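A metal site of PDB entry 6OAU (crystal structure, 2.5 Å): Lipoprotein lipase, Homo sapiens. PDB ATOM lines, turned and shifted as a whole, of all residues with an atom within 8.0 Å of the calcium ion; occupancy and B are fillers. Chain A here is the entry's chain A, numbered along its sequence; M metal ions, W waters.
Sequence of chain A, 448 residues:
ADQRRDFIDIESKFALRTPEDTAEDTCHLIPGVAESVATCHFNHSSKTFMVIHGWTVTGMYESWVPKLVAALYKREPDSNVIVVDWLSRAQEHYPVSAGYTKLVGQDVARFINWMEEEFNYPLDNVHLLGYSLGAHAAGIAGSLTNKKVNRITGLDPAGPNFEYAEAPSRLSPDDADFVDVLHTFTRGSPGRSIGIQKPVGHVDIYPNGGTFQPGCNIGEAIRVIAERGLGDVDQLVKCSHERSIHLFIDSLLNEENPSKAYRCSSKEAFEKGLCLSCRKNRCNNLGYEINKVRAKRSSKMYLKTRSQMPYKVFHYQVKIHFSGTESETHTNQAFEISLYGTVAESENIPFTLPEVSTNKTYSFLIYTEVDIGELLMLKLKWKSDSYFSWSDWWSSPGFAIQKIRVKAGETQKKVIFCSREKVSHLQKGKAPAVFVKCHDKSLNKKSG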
ATOM      1  N   LYS A 102      -7.302  24.507 -31.389  1.00  0.00           N
ATOM      2  CA  LYS A 102      -8.679  24.911 -31.104  1.00  0.00           C
ATOM      3  C   LYS A 102      -9.430  25.203 -32.409  1.00  0.00           C
ATOM      4  O   LYS A 102     -10.568  24.786 -32.545  1.00  0.00           O
ATOM      5  CB  LYS A 102      -8.774  26.086 -30.125  1.00  0.00           C
ATOM      6  CG  LYS A 102      -8.872  25.708 -28.626  1.00  0.00           C
ATOM      7  CD  LYS A 102     -10.216  26.092 -27.994  1.00  0.00           C
ATOM      8  CE  LYS A 102     -10.894  24.910 -27.346  1.00  0.00           C
ATOM      9  NZ  LYS A 102     -12.366  24.896 -27.621  1.00  0.00           N
ATOM     10  N   ALA A 135      -3.678  15.134 -31.508  1.00  0.00           N
ATOM     11  CA  ALA A 135      -4.439  14.429 -30.465  1.00  0.00           C
ATOM     12  C   ALA A 135      -5.267  15.455 -29.692  1.00  0.00           C
ATOM     13  O   ALA A 135      -6.433  15.223 -29.399  1.00  0.00           O
ATOM     14  CB  ALA A 135      -3.511  13.683 -29.534  1.00  0.00           C
ATOM     15  N   HIS A 136      -4.693  16.632 -29.449  1.00  0.00           N
ATOM     16  CA  HIS A 136      -5.348  17.752 -28.783  1.00  0.00           C
ATOM     17  C   HIS A 136      -6.410  18.340 -29.654  1.00  0.00           C
ATOM     18  O   HIS A 136      -7.514  18.610 -29.158  1.00  0.00           O
ATOM     19  CB  HIS A 136      -4.329  18.791 -28.340  1.00  0.00           C
ATOM     20  CG  HIS A 136      -3.410  18.248 -27.299  1.00  0.00           C
ATOM     21  ND1 HIS A 136      -3.885  17.803 -26.067  1.00  0.00           N
ATOM     22  CD2 HIS A 136      -2.089  17.970 -27.375  1.00  0.00           C
ATOM     23  CE1 HIS A 136      -2.837  17.336 -25.428  1.00  0.00           C
ATOM     24  NE2 HIS A 136      -1.735  17.408 -26.180  1.00  0.00           N
ATOM     25  N   ALA A 138      -7.874  16.624 -32.050  1.00  0.00           N
ATOM     26  CA  ALA A 138      -8.851  15.509 -32.141  1.00  0.00           C
ATOM     27  C   ALA A 138      -9.807  15.587 -30.931  1.00  0.00           C
ATOM     28  O   ALA A 138     -11.015  15.521 -31.113  1.00  0.00           O
ATOM     29  CB  ALA A 138      -8.142  14.163 -32.150  1.00  0.00           C
ATOM     30  N   GLY A 139      -9.253  15.800 -29.750  1.00  0.00           N
ATOM     31  CA  GLY A 139     -10.003  15.983 -28.511  1.00  0.00           C
ATOM     32  C   GLY A 139     -10.875  17.215 -28.537  1.00  0.00           C
ATOM     33  O   GLY A 139     -12.051  17.124 -28.187  1.00  0.00           O
ATOM     34  N   ILE A 140     -10.341  18.370 -29.019  1.00  0.00           N
ATOM     35  CA  ILE A 140     -11.139  19.624 -29.163  1.00  0.00           C
ATOM     36  C   ILE A 140     -12.337  19.366 -30.111  1.00  0.00           C
ATOM     37  O   ILE A 140     -13.476  19.648 -29.740  1.00  0.00           O
ATOM     38  CB  ILE A 140     -10.275  20.835 -29.551  1.00  0.00           C
ATOM     39  CG1 ILE A 140      -9.444  21.301 -28.324  1.00  0.00           C
ATOM     40  CG2 ILE A 140     -11.106  21.995 -30.119  1.00  0.00           C
ATOM     41  CD1 ILE A 140      -8.042  21.989 -28.647  1.00  0.00           C
ATOM     42  N   ALA A 141     -12.070  18.737 -31.278  1.00  0.00           N
ATOM     43  CA  ALA A 141     -13.081  18.319 -32.239  1.00  0.00           C
ATOM     44  C   ALA A 141     -14.171  17.467 -31.565  1.00  0.00           C
ATOM     45  O   ALA A 141     -15.343  17.817 -31.652  1.00  0.00           O
ATOM     46  CB  ALA A 141     -12.430  17.535 -33.374  1.00  0.00           C
ATOM     47  N   GLY A 142     -13.753  16.403 -30.853  1.00  0.00           N
ATOM     48  CA  GLY A 142     -14.640  15.475 -30.155  1.00  0.00           C
ATOM     49  C   GLY A 142     -15.615  16.131 -29.185  1.00  0.00           C
ATOM     50  O   GLY A 142     -16.759  15.687 -29.053  1.00  0.00           O
ATOM     51  N   SER A 143     -15.170  17.205 -28.530  1.00  0.00           N
ATOM     52  CA  SER A 143     -15.928  18.014 -27.573  1.00  0.00           C
ATOM     53  C   SER A 143     -16.975  18.946 -28.240  1.00  0.00           C
ATOM     54  O   SER A 143     -17.817  19.518 -27.534  1.00  0.00           O
ATOM     55  CB  SER A 143     -14.961  18.852 -26.736  1.00  0.00           C
ATOM     56  OG  SER A 143     -14.616  20.079 -27.368  1.00  0.00           O
ATOM     57  N   LEU A 144     -16.903  19.126 -29.587  1.00  0.00           N
ATOM     58  CA  LEU A 144     -17.757  20.034 -30.362  1.00  0.00           C
ATOM     59  C   LEU A 144     -18.689  19.360 -31.344  1.00  0.00           C
ATOM     60  O   LEU A 144     -19.427  20.029 -32.087  1.00  0.00           O
ATOM     61  CB  LEU A 144     -16.920  21.096 -31.082  1.00  0.00           C
ATOM     62  CG  LEU A 144     -16.172  22.113 -30.206  1.00  0.00           C
ATOM     63  CD1 LEU A 144     -15.188  22.907 -31.033  1.00  0.00           C
ATOM     64  CD2 LEU A 144     -17.132  23.038 -29.456  1.00  0.00           C
ATOM     65  N   ILE A 152     -11.149   8.036 -30.104  1.00  0.00           N
ATOM     66  CA  ILE A 152     -10.034   8.957 -30.312  1.00  0.00           C
ATOM     67  C   ILE A 152      -8.864   8.186 -29.811  1.00  0.00           C
ATOM     68  O   ILE A 152      -8.903   7.650 -28.707  1.00  0.00           O
ATOM     69  CB  ILE A 152     -10.083  10.351 -29.592  1.00  0.00           C
ATOM     70  CG1 ILE A 152     -11.295  11.199 -30.048  1.00  0.00           C
ATOM     71  CG2 ILE A 152      -8.770  11.124 -29.856  1.00  0.00           C
ATOM     72  CD1 ILE A 152     -11.518  12.507 -29.210  1.00  0.00           C
ATOM     73  N   GLU A 166      -6.614  22.879 -19.066  1.00  0.00           N
ATOM     74  CA  GLU A 166      -7.896  22.356 -18.627  1.00  0.00           C
ATOM     75  C   GLU A 166      -8.477  21.493 -19.739  1.00  0.00           C
ATOM     76  O   GLU A 166      -8.171  21.738 -20.912  1.00  0.00           O
ATOM     77  CB  GLU A 166      -8.850  23.511 -18.279  1.00  0.00           C
ATOM     78  CG  GLU A 166      -8.737  23.955 -16.836  1.00  0.00           C
ATOM     79  CD  GLU A 166      -9.052  22.884 -15.806  1.00  0.00           C
ATOM     80  OE1 GLU A 166     -10.114  22.229 -15.915  1.00  0.00           O
ATOM     81  OE2 GLU A 166      -8.225  22.698 -14.878  1.00  0.00           O
ATOM     82  N   ALA A 167      -9.326  20.498 -19.361  1.00  0.00           N
ATOM     83  CA  ALA A 167      -9.978  19.549 -20.266  1.00  0.00           C
ATOM     84  C   ALA A 167     -10.517  20.145 -21.583  1.00  0.00           C
ATOM     85  O   ALA A 167     -10.344  19.472 -22.610  1.00  0.00           O
ATOM     86  CB  ALA A 167     -11.077  18.793 -19.547  1.00  0.00           C
ATOM     87  N   PRO A 168     -11.114  21.377 -21.655  1.00  0.00           N
ATOM     88  CA  PRO A 168     -11.589  21.861 -22.965  1.00  0.00           C
ATOM     89  C   PRO A 168     -10.492  22.183 -23.953  1.00  0.00           C
ATOM     90  O   PRO A 168     -10.757  22.191 -25.141  1.00  0.00           O
ATOM     91  CB  PRO A 168     -12.380  23.138 -22.632  1.00  0.00           C
ATOM     92  CG  PRO A 168     -12.537  23.164 -21.171  1.00  0.00           C
ATOM     93  CD  PRO A 168     -11.443  22.353 -20.590  1.00  0.00           C
ATOM     94  N   SER A 169      -9.279  22.466 -23.454  1.00  0.00           N
ATOM     95  CA  SER A 169      -8.120  22.904 -24.221  1.00  0.00           C
ATOM     96  C   SER A 169      -7.176  21.776 -24.649  1.00  0.00           C
ATOM     97  O   SER A 169      -6.105  22.043 -25.186  1.00  0.00           O
ATOM     98  CB  SER A 169      -7.328  23.936 -23.410  1.00  0.00           C
ATOM     99  OG  SER A 169      -8.127  25.024 -22.937  1.00  0.00           O
ATOM    100  N   ARG A 170      -7.531  20.534 -24.397  1.00  0.00           N
ATOM    101  CA  ARG A 170      -6.682  19.371 -24.673  1.00  0.00           C
ATOM    102  C   ARG A 170      -7.519  18.146 -24.861  1.00  0.00           C
ATOM    103  O   ARG A 170      -8.738  18.201 -24.714  1.00  0.00           O
ATOM    104  CB  ARG A 170      -5.731  19.148 -23.480  1.00  0.00           C
ATOM    105  CG  ARG A 170      -6.456  18.921 -22.143  1.00  0.00           C
ATOM    106  CD  ARG A 170      -5.572  18.194 -21.169  1.00  0.00           C
ATOM    107  NE  ARG A 170      -6.124  18.252 -19.811  1.00  0.00           N
ATOM    108  CZ  ARG A 170      -6.934  17.334 -19.292  1.00  0.00           C
ATOM    109  NH1 ARG A 170      -7.373  17.463 -18.048  1.00  0.00           N
ATOM    110  NH2 ARG A 170      -7.291  16.268 -19.994  1.00  0.00           N
ATOM    111  N   LEU A 171      -6.871  16.992 -25.098  1.00  0.00           N
ATOM    112  CA  LEU A 171      -7.529  15.692 -25.144  1.00  0.00           C
ATOM    113  C   LEU A 171      -7.958  15.350 -23.727  1.00  0.00           C
ATOM    114  O   LEU A 171      -7.201  15.556 -22.795  1.00  0.00           O
ATOM    115  CB  LEU A 171      -6.536  14.599 -25.661  1.00  0.00           C
ATOM    116  CG  LEU A 171      -7.105  13.192 -25.916  1.00  0.00           C
ATOM    117  CD1 LEU A 171      -8.261  13.236 -26.852  1.00  0.00           C
ATOM    118  CD2 LEU A 171      -6.024  12.255 -26.452  1.00  0.00           C
ATOM    119  N   SER A 172      -9.177  14.898 -23.563  1.00  0.00           N
ATOM    120  CA  SER A 172      -9.740  14.489 -22.271  1.00  0.00           C
ATOM    121  C   SER A 172     -10.626  13.246 -22.496  1.00  0.00           C
ATOM    122  O   SER A 172     -11.077  13.045 -23.638  1.00  0.00           O
ATOM    123  CB  SER A 172     -10.522  15.646 -21.636  1.00  0.00           C
ATOM    124  OG  SER A 172     -11.938  15.519 -21.748  1.00  0.00           O
ATOM    125  N   PRO A 173     -10.924  12.416 -21.450  1.00  0.00           N
ATOM    126  CA  PRO A 173     -11.791  11.240 -21.684  1.00  0.00           C
ATOM    127  C   PRO A 173     -13.218  11.571 -22.108  1.00  0.00           C
ATOM    128  O   PRO A 173     -13.895  10.722 -22.670  1.00  0.00           O
ATOM    129  CB  PRO A 173     -11.772  10.528 -20.329  1.00  0.00           C
ATOM    130  CG  PRO A 173     -10.571  11.058 -19.623  1.00  0.00           C
ATOM    131  CD  PRO A 173     -10.484  12.475 -20.046  1.00  0.00           C
ATOM    132  N   ASP A 174     -13.674  12.805 -21.852  1.00  0.00           N
ATOM    133  CA  ASP A 174     -15.018  13.309 -22.162  1.00  0.00           C
ATOM    134  C   ASP A 174     -15.235  13.605 -23.658  1.00  0.00           C
ATOM    135  O   ASP A 174     -16.369  13.846 -24.054  1.00  0.00           O
ATOM    136  CB  ASP A 174     -15.308  14.597 -21.362  1.00  0.00           C
ATOM    137  CG  ASP A 174     -14.730  14.632 -19.968  1.00  0.00           C
ATOM    138  OD1 ASP A 174     -15.229  13.864 -19.093  1.00  0.00           O
ATOM    139  OD2 ASP A 174     -13.770  15.413 -19.733  1.00  0.00           O
ATOM    140  N   ASP A 175     -14.157  13.612 -24.454  1.00  0.00           N
ATOM    141  CA  ASP A 175     -14.168  14.003 -25.871  1.00  0.00           C
ATOM    142  C   ASP A 175     -14.747  12.961 -26.823  1.00  0.00           C
ATOM    143  O   ASP A 175     -15.218  13.316 -27.896  1.00  0.00           O
ATOM    144  CB  ASP A 175     -12.767  14.438 -26.286  1.00  0.00           C
ATOM    145  CG  ASP A 175     -12.293  15.650 -25.508  1.00  0.00           C
ATOM    146  OD1 ASP A 175     -13.162  16.376 -24.956  1.00  0.00           O
ATOM    147  OD2 ASP A 175     -11.073  15.879 -25.439  1.00  0.00           O
ATOM    148  N   ALA A 176     -14.729  11.672 -26.433  1.00  0.00           N
ATOM    149  CA  ALA A 176     -15.271  10.558 -27.210  1.00  0.00           C
ATOM    150  C   ALA A 176     -15.803   9.505 -26.253  1.00  0.00           C
ATOM    151  O   ALA A 176     -15.551   9.589 -25.061  1.00  0.00           O
ATOM    152  CB  ALA A 176     -14.177   9.959 -28.067  1.00  0.00           C
ATOM    153  N   VAL A 200      -4.708  11.240 -20.050  1.00  0.00           N
ATOM    154  CA  VAL A 200      -5.735  12.083 -20.705  1.00  0.00           C
ATOM    155  C   VAL A 200      -6.871  11.265 -21.368  1.00  0.00           C
ATOM    156  O   VAL A 200      -7.761  11.844 -21.988  1.00  0.00           O
ATOM    157  CB  VAL A 200      -5.118  13.122 -21.712  1.00  0.00           C
ATOM    158  CG1 VAL A 200      -4.259  14.147 -21.001  1.00  0.00           C
ATOM    159  CG2 VAL A 200      -4.341  12.436 -22.840  1.00  0.00           C
HETATM  160 CA    CA M   1     -11.275  18.029 -24.224  1.00  0.00          CA
HETATM  161  O   HOH W   1     -14.202  18.435 -22.919  1.00  0.00           O
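OG of Ser 172 sits at hydrogen-bond distance from OD2 of Asp 174 (2.7 Å). OD2 of Asp 175 lies close to N of Ser 172, 2.8 Å away.
Ser 172 touches the calcium ion (OG to CA, 3.6 Å). Four residues have an atom within 4 Å of the calcium ion: Ala 167, Arg 170, Ser 172 and Asp 175. The nearest printed residue that does not touch the calcium ion is Pro 168 (4.05 Å).
The calcium ion is bound by the backbone carbonyl oxygen (O) of Ala 167, the side-chain carboxylate (OD2) of Asp 175, the backbone carbonyl oxygen (O) of Arg 170 and the side-chain carboxylate (OD1) of Asp 175. The calcium ion has four donor atoms within binding distance.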
